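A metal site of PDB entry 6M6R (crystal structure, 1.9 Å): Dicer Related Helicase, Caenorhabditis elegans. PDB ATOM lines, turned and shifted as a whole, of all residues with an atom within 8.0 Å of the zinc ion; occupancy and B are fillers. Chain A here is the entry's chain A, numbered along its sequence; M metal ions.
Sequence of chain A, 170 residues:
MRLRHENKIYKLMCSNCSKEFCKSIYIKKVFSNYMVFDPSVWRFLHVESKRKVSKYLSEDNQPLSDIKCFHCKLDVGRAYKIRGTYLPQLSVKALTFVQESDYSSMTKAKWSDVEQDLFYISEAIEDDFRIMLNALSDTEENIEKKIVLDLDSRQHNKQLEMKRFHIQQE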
ATOM      1  N   MET A  13       1.602  10.474  15.625  1.00  0.00           N
ATOM      2  CA  MET A  13       2.248   9.423  14.857  1.00  0.00           C
ATOM      3  C   MET A  13       3.656   9.817  14.451  1.00  0.00           C
ATOM      4  O   MET A  13       3.985  11.001  14.334  1.00  0.00           O
ATOM      5  CB  MET A  13       1.370   9.076  13.645  1.00  0.00           C
ATOM      6  CG  MET A  13       0.083   8.360  14.121  1.00  0.00           C
ATOM      7  SD  MET A  13      -1.225   8.370  12.900  1.00  0.00           S
ATOM      8  CE  MET A  13      -0.274   8.219  11.386  1.00  0.00           C
ATOM      9  N   CYS A  14       4.511   8.807  14.283  1.00  0.00           N
ATOM     10  CA  CYS A  14       5.869   9.040  13.769  1.00  0.00           C
ATOM     11  C   CYS A  14       5.777   9.639  12.375  1.00  0.00           C
ATOM     12  O   CYS A  14       5.129   9.073  11.482  1.00  0.00           O
ATOM     13  CB  CYS A  14       6.650   7.714  13.729  1.00  0.00           C
ATOM     14  SG  CYS A  14       8.347   7.890  13.114  1.00  0.00           S
ATOM     15  N   SER A  15       6.421  10.796  12.170  1.00  0.00           N
ATOM     16  CA  SER A  15       6.287  11.378  10.846  1.00  0.00           C
ATOM     17  C   SER A  15       7.060  10.619   9.789  1.00  0.00           C
ATOM     18  O   SER A  15       6.833  10.845   8.600  1.00  0.00           O
ATOM     19  CB  SER A  15       6.725  12.849  10.861  1.00  0.00           C
ATOM     20  OG  SER A  15       8.097  12.901  11.193  1.00  0.00           O
ATOM     21  N   ASN A  16       7.955   9.697  10.191  1.00  0.00           N
ATOM     22  CA  ASN A  16       8.701   8.892   9.236  1.00  0.00           C
ATOM     23  C   ASN A  16       7.997   7.587   8.843  1.00  0.00           C
ATOM     24  O   ASN A  16       7.910   7.247   7.656  1.00  0.00           O
ATOM     25  CB  ASN A  16      10.106   8.586   9.790  1.00  0.00           C
ATOM     26  CG  ASN A  16      11.024   7.939   8.738  1.00  0.00           C
ATOM     27  OD1 ASN A  16      10.979   8.301   7.560  1.00  0.00           O
ATOM     28  ND2 ASN A  16      11.826   6.972   9.155  1.00  0.00           N
ATOM     29  N   CYS A  17       7.487   6.831   9.813  1.00  0.00           N
ATOM     30  CA  CYS A  17       6.932   5.517   9.495  1.00  0.00           C
ATOM     31  C   CYS A  17       5.444   5.390   9.801  1.00  0.00           C
ATOM     32  O   CYS A  17       4.849   4.347   9.495  1.00  0.00           O
ATOM     33  CB  CYS A  17       7.728   4.434  10.258  1.00  0.00           C
ATOM     34  SG  CYS A  17       7.351   4.308  12.014  1.00  0.00           S
ATOM     35  N   SER A  18       4.834   6.428  10.384  1.00  0.00           N
ATOM     36  CA  SER A  18       3.415   6.545  10.720  1.00  0.00           C
ATOM     37  C   SER A  18       2.962   5.637  11.872  1.00  0.00           C
ATOM     38  O   SER A  18       1.754   5.513  12.099  1.00  0.00           O
ATOM     39  CB  SER A  18       2.525   6.300   9.483  1.00  0.00           C
ATOM     40  OG  SER A  18       2.215   4.920   9.352  1.00  0.00           O
ATOM     41  N   LYS A  19       3.876   5.045  12.640  1.00  0.00           N
ATOM     42  CA  LYS A  19       3.460   4.317  13.851  1.00  0.00           C
ATOM     43  C   LYS A  19       2.929   5.292  14.899  1.00  0.00           C
ATOM     44  O   LYS A  19       3.484   6.370  15.082  1.00  0.00           O
ATOM     45  CB  LYS A  19       4.608   3.500  14.437  1.00  0.00           C
ATOM     46  CG  LYS A  19       5.058   2.347  13.555  1.00  0.00           C
ATOM     47  CD  LYS A  19       4.031   1.219  13.456  1.00  0.00           C
ATOM     48  CE  LYS A  19       4.706  -0.091  13.007  1.00  0.00           C
ATOM     49  NZ  LYS A  19       3.812  -0.969  12.175  1.00  0.00           N
ATOM     50  N   GLU A  20       1.845   4.913  15.582  1.00  0.00           N
ATOM     51  CA  GLU A  20       1.222   5.784  16.562  1.00  0.00           C
ATOM     52  C   GLU A  20       1.911   5.657  17.918  1.00  0.00           C
ATOM     53  O   GLU A  20       2.059   4.546  18.444  1.00  0.00           O
ATOM     54  CB  GLU A  20      -0.260   5.447  16.696  1.00  0.00           C
ATOM     55  CG  GLU A  20      -0.933   6.241  17.803  1.00  0.00           C
ATOM     56  CD  GLU A  20      -2.394   5.850  18.007  1.00  0.00           C
ATOM     57  OE1 GLU A  20      -2.956   5.155  17.136  1.00  0.00           O
ATOM     58  OE2 GLU A  20      -2.957   6.231  19.057  1.00  0.00           O
ATOM     59  N   PHE A  21       2.316   6.798  18.489  1.00  0.00           N
ATOM     60  CA  PHE A  21       2.922   6.763  19.820  1.00  0.00           C
ATOM     61  C   PHE A  21       1.872   6.831  20.914  1.00  0.00           C
ATOM     62  O   PHE A  21       1.894   6.009  21.843  1.00  0.00           O
ATOM     63  CB  PHE A  21       3.904   7.927  19.981  1.00  0.00           C
ATOM     64  CG  PHE A  21       5.084   7.850  19.064  1.00  0.00           C
ATOM     65  CD1 PHE A  21       5.843   6.690  18.971  1.00  0.00           C
ATOM     66  CD2 PHE A  21       5.437   8.938  18.268  1.00  0.00           C
ATOM     67  CE1 PHE A  21       6.928   6.629  18.117  1.00  0.00           C
ATOM     68  CE2 PHE A  21       6.522   8.877  17.414  1.00  0.00           C
ATOM     69  CZ  PHE A  21       7.277   7.709  17.347  1.00  0.00           C
ATOM     70  N   PHE A  44       6.639   1.869  22.458  1.00  0.00           N
ATOM     71  CA  PHE A  44       6.867   2.336  21.095  1.00  0.00           C
ATOM     72  C   PHE A  44       8.147   3.132  20.947  1.00  0.00           C
ATOM     73  O   PHE A  44       8.415   3.629  19.846  1.00  0.00           O
ATOM     74  CB  PHE A  44       5.652   3.152  20.646  1.00  0.00           C
ATOM     75  CG  PHE A  44       4.350   2.415  20.837  1.00  0.00           C
ATOM     76  CD1 PHE A  44       4.123   1.224  20.149  1.00  0.00           C
ATOM     77  CD2 PHE A  44       3.395   2.858  21.727  1.00  0.00           C
ATOM     78  CE1 PHE A  44       2.943   0.503  20.336  1.00  0.00           C
ATOM     79  CE2 PHE A  44       2.215   2.137  21.914  1.00  0.00           C
ATOM     80  CZ  PHE A  44       1.999   0.964  21.217  1.00  0.00           C
ATOM     81  N   LYS A  68      14.140   7.210  20.330  1.00  0.00           N
ATOM     82  CA  LYS A  68      13.893   7.000  18.914  1.00  0.00           C
ATOM     83  C   LYS A  68      12.632   6.170  18.758  1.00  0.00           C
ATOM     84  O   LYS A  68      12.224   5.443  19.664  1.00  0.00           O
ATOM     85  CB  LYS A  68      15.073   6.263  18.232  1.00  0.00           C
ATOM     86  CG  LYS A  68      16.445   6.910  18.459  1.00  0.00           C
ATOM     87  CD  LYS A  68      17.542   6.022  17.890  1.00  0.00           C
ATOM     88  CE  LYS A  68      18.847   6.773  17.786  1.00  0.00           C
ATOM     89  NZ  LYS A  68      19.372   7.120  19.139  1.00  0.00           N
ATOM     90  N   CYS A  69      12.023   6.289  17.577  1.00  0.00           N
ATOM     91  CA  CYS A  69      10.914   5.426  17.227  1.00  0.00           C
ATOM     92  C   CYS A  69      11.394   3.979  17.257  1.00  0.00           C
ATOM     93  O   CYS A  69      12.405   3.643  16.624  1.00  0.00           O
ATOM     94  CB  CYS A  69      10.356   5.797  15.844  1.00  0.00           C
ATOM     95  SG  CYS A  69       9.088   4.681  15.238  1.00  0.00           S
ATOM     96  N   PHE A  70      10.688   3.136  17.997  1.00  0.00           N
ATOM     97  CA  PHE A  70      11.131   1.740  18.094  1.00  0.00           C
ATOM     98  C   PHE A  70      11.068   1.056  16.745  1.00  0.00           C
ATOM     99  O   PHE A  70      11.868   0.161  16.452  1.00  0.00           O
ATOM    100  CB  PHE A  70      10.278   0.971  19.099  1.00  0.00           C
ATOM    101  CG  PHE A  70      10.907  -0.337  19.530  1.00  0.00           C
ATOM    102  CD1 PHE A  70      11.906  -0.347  20.503  1.00  0.00           C
ATOM    103  CD2 PHE A  70      10.530  -1.527  18.935  1.00  0.00           C
ATOM    104  CE1 PHE A  70      12.504  -1.538  20.895  1.00  0.00           C
ATOM    105  CE2 PHE A  70      11.131  -2.737  19.315  1.00  0.00           C
ATOM    106  CZ  PHE A  70      12.118  -2.742  20.295  1.00  0.00           C
ATOM    107  N   HIS A  71      10.152   1.489  15.878  1.00  0.00           N
ATOM    108  CA  HIS A  71      10.004   0.821  14.593  1.00  0.00           C
ATOM    109  C   HIS A  71      11.109   1.235  13.626  1.00  0.00           C
ATOM    110  O   HIS A  71      11.845   0.391  13.113  1.00  0.00           O
ATOM    111  CB  HIS A  71       8.639   1.131  13.987  1.00  0.00           C
ATOM    112  CG  HIS A  71       8.337   0.336  12.751  1.00  0.00           C
ATOM    113  ND1 HIS A  71       8.055  -1.010  12.784  1.00  0.00           N
ATOM    114  CD2 HIS A  71       8.274   0.700  11.451  1.00  0.00           C
ATOM    115  CE1 HIS A  71       7.838  -1.445  11.562  1.00  0.00           C
ATOM    116  NE2 HIS A  71       7.970  -0.430  10.722  1.00  0.00           N
ATOM    117  N   CYS A  72      11.225   2.536  13.358  1.00  0.00           N
ATOM    118  CA  CYS A  72      12.081   3.032  12.275  1.00  0.00           C
ATOM    119  C   CYS A  72      13.337   3.720  12.770  1.00  0.00           C
ATOM    120  O   CYS A  72      14.171   4.112  11.952  1.00  0.00           O
ATOM    121  CB  CYS A  72      11.280   3.990  11.371  1.00  0.00           C
ATOM    122  SG  CYS A  72      11.024   5.652  12.068  1.00  0.00           S
ATOM    123  N   LYS A  73      13.483   3.900  14.085  1.00  0.00           N
ATOM    124  CA  LYS A  73      14.668   4.488  14.726  1.00  0.00           C
ATOM    125  C   LYS A  73      14.860   5.980  14.414  1.00  0.00           C
ATOM    126  O   LYS A  73      15.914   6.534  14.739  1.00  0.00           O
ATOM    127  CB  LYS A  73      15.930   3.675  14.387  1.00  0.00           C
ATOM    128  CG  LYS A  73      16.306   2.677  15.498  1.00  0.00           C
ATOM    129  CD  LYS A  73      15.182   1.671  15.813  1.00  0.00           C
ATOM    130  CE  LYS A  73      15.664   0.278  16.246  1.00  0.00           C
ATOM    131  NZ  LYS A  73      14.771  -0.348  17.300  1.00  0.00           N
ATOM    132  N   LEU A  74      13.857   6.664  13.866  1.00  0.00           N
ATOM    133  CA  LEU A  74      13.938   8.126  13.780  1.00  0.00           C
ATOM    134  C   LEU A  74      14.131   8.709  15.182  1.00  0.00           C
ATOM    135  O   LEU A  74      13.550   8.231  16.153  1.00  0.00           O
ATOM    136  CB  LEU A  74      12.653   8.681  13.147  1.00  0.00           C
ATOM    137  CG  LEU A  74      12.429  10.220  13.135  1.00  0.00           C
ATOM    138  CD1 LEU A  74      13.219  10.847  11.974  1.00  0.00           C
ATOM    139  CD2 LEU A  74      10.909  10.615  13.101  1.00  0.00           C
ATOM    140  N   ASP A  75      14.969   9.745  15.289  1.00  0.00           N
ATOM    141  CA  ASP A  75      15.067  10.497  16.538  1.00  0.00           C
ATOM    142  C   ASP A  75      13.787  11.263  16.771  1.00  0.00           C
ATOM    143  O   ASP A  75      13.406  12.115  15.953  1.00  0.00           O
ATOM    144  CB  ASP A  75      16.280  11.439  16.480  1.00  0.00           C
ATOM    145  CG  ASP A  75      16.470  12.243  17.766  1.00  0.00           C
ATOM    146  OD1 ASP A  75      15.903  11.906  18.825  1.00  0.00           O
ATOM    147  OD2 ASP A  75      17.228  13.239  17.714  1.00  0.00           O
ATOM    148  N   VAL A  76      13.088  10.974  17.866  1.00  0.00           N
ATOM    149  CA  VAL A  76      11.792  11.596  18.130  1.00  0.00           C
ATOM    150  C   VAL A  76      11.786  12.413  19.424  1.00  0.00           C
ATOM    151  O   VAL A  76      10.744  12.978  19.767  1.00  0.00           O
ATOM    152  CB  VAL A  76      10.646  10.549  18.146  1.00  0.00           C
ATOM    153  CG1 VAL A  76      10.474   9.914  16.755  1.00  0.00           C
ATOM    154  CG2 VAL A  76      10.895   9.444  19.160  1.00  0.00           C
ATOM    155  N   ALA A  94       8.931  15.863  15.025  1.00  0.00           N
ATOM    156  CA  ALA A  94       8.990  14.458  14.629  1.00  0.00           C
ATOM    157  C   ALA A  94       7.614  13.804  14.533  1.00  0.00           C
ATOM    158  O   ALA A  94       7.542  12.615  14.207  1.00  0.00           O
ATOM    159  CB  ALA A  94       9.873  13.693  15.618  1.00  0.00           C
HETATM  160 ZN    ZN M   1       8.924   5.630  13.030  1.00  0.00          ZN
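The zinc ion is bound by the side-chain sulfur (SG) of Cys 17 (2.3 Å), the side-chain sulfur (SG) of Cys 72 (2.3 Å), the side-chain sulfur (SG) of Cys 14 (2.3 Å) and the side-chain sulfur (SG) of Cys 69 (2.4 Å).
The zinc ion has four donor atoms within binding distance.
The side-chain sulfur of Cys 72 sits close to the backbone NH of Leu 74, 3.5 Å away.
N of Lys 19 sits close to SG of Cys 17, at 3.6 Å.
The backbone carbonyl oxygen (O) of Lys 19 lies within hydrogen-bond range of the backbone NH (N) of Cys 14, at 2.8 Å.
ND2 of Asn 16 sits close to SG of Cys 72, 3.3 Å away.
The backbone NH (N) of Asn 16 lies close to the side-chain sulfur (SG) of Cys 14, 3.5 Å away.
N of Cys 69 sits at hydrogen-bond distance from O of Leu 74 (2.9 Å).
N of His 71 sits close to SG of Cys 69 (3.4 Å).
Four residues have an atom within 4 Å of the zinc ion: Cys 14, Cys 17, Cys 69 and Cys 72.
Along chain A the residues within 4 Å of the zinc ion span positions 14 to 72.
The nearest printed residue that does not touch the zinc ion is Asn 16 (4.5 Å).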
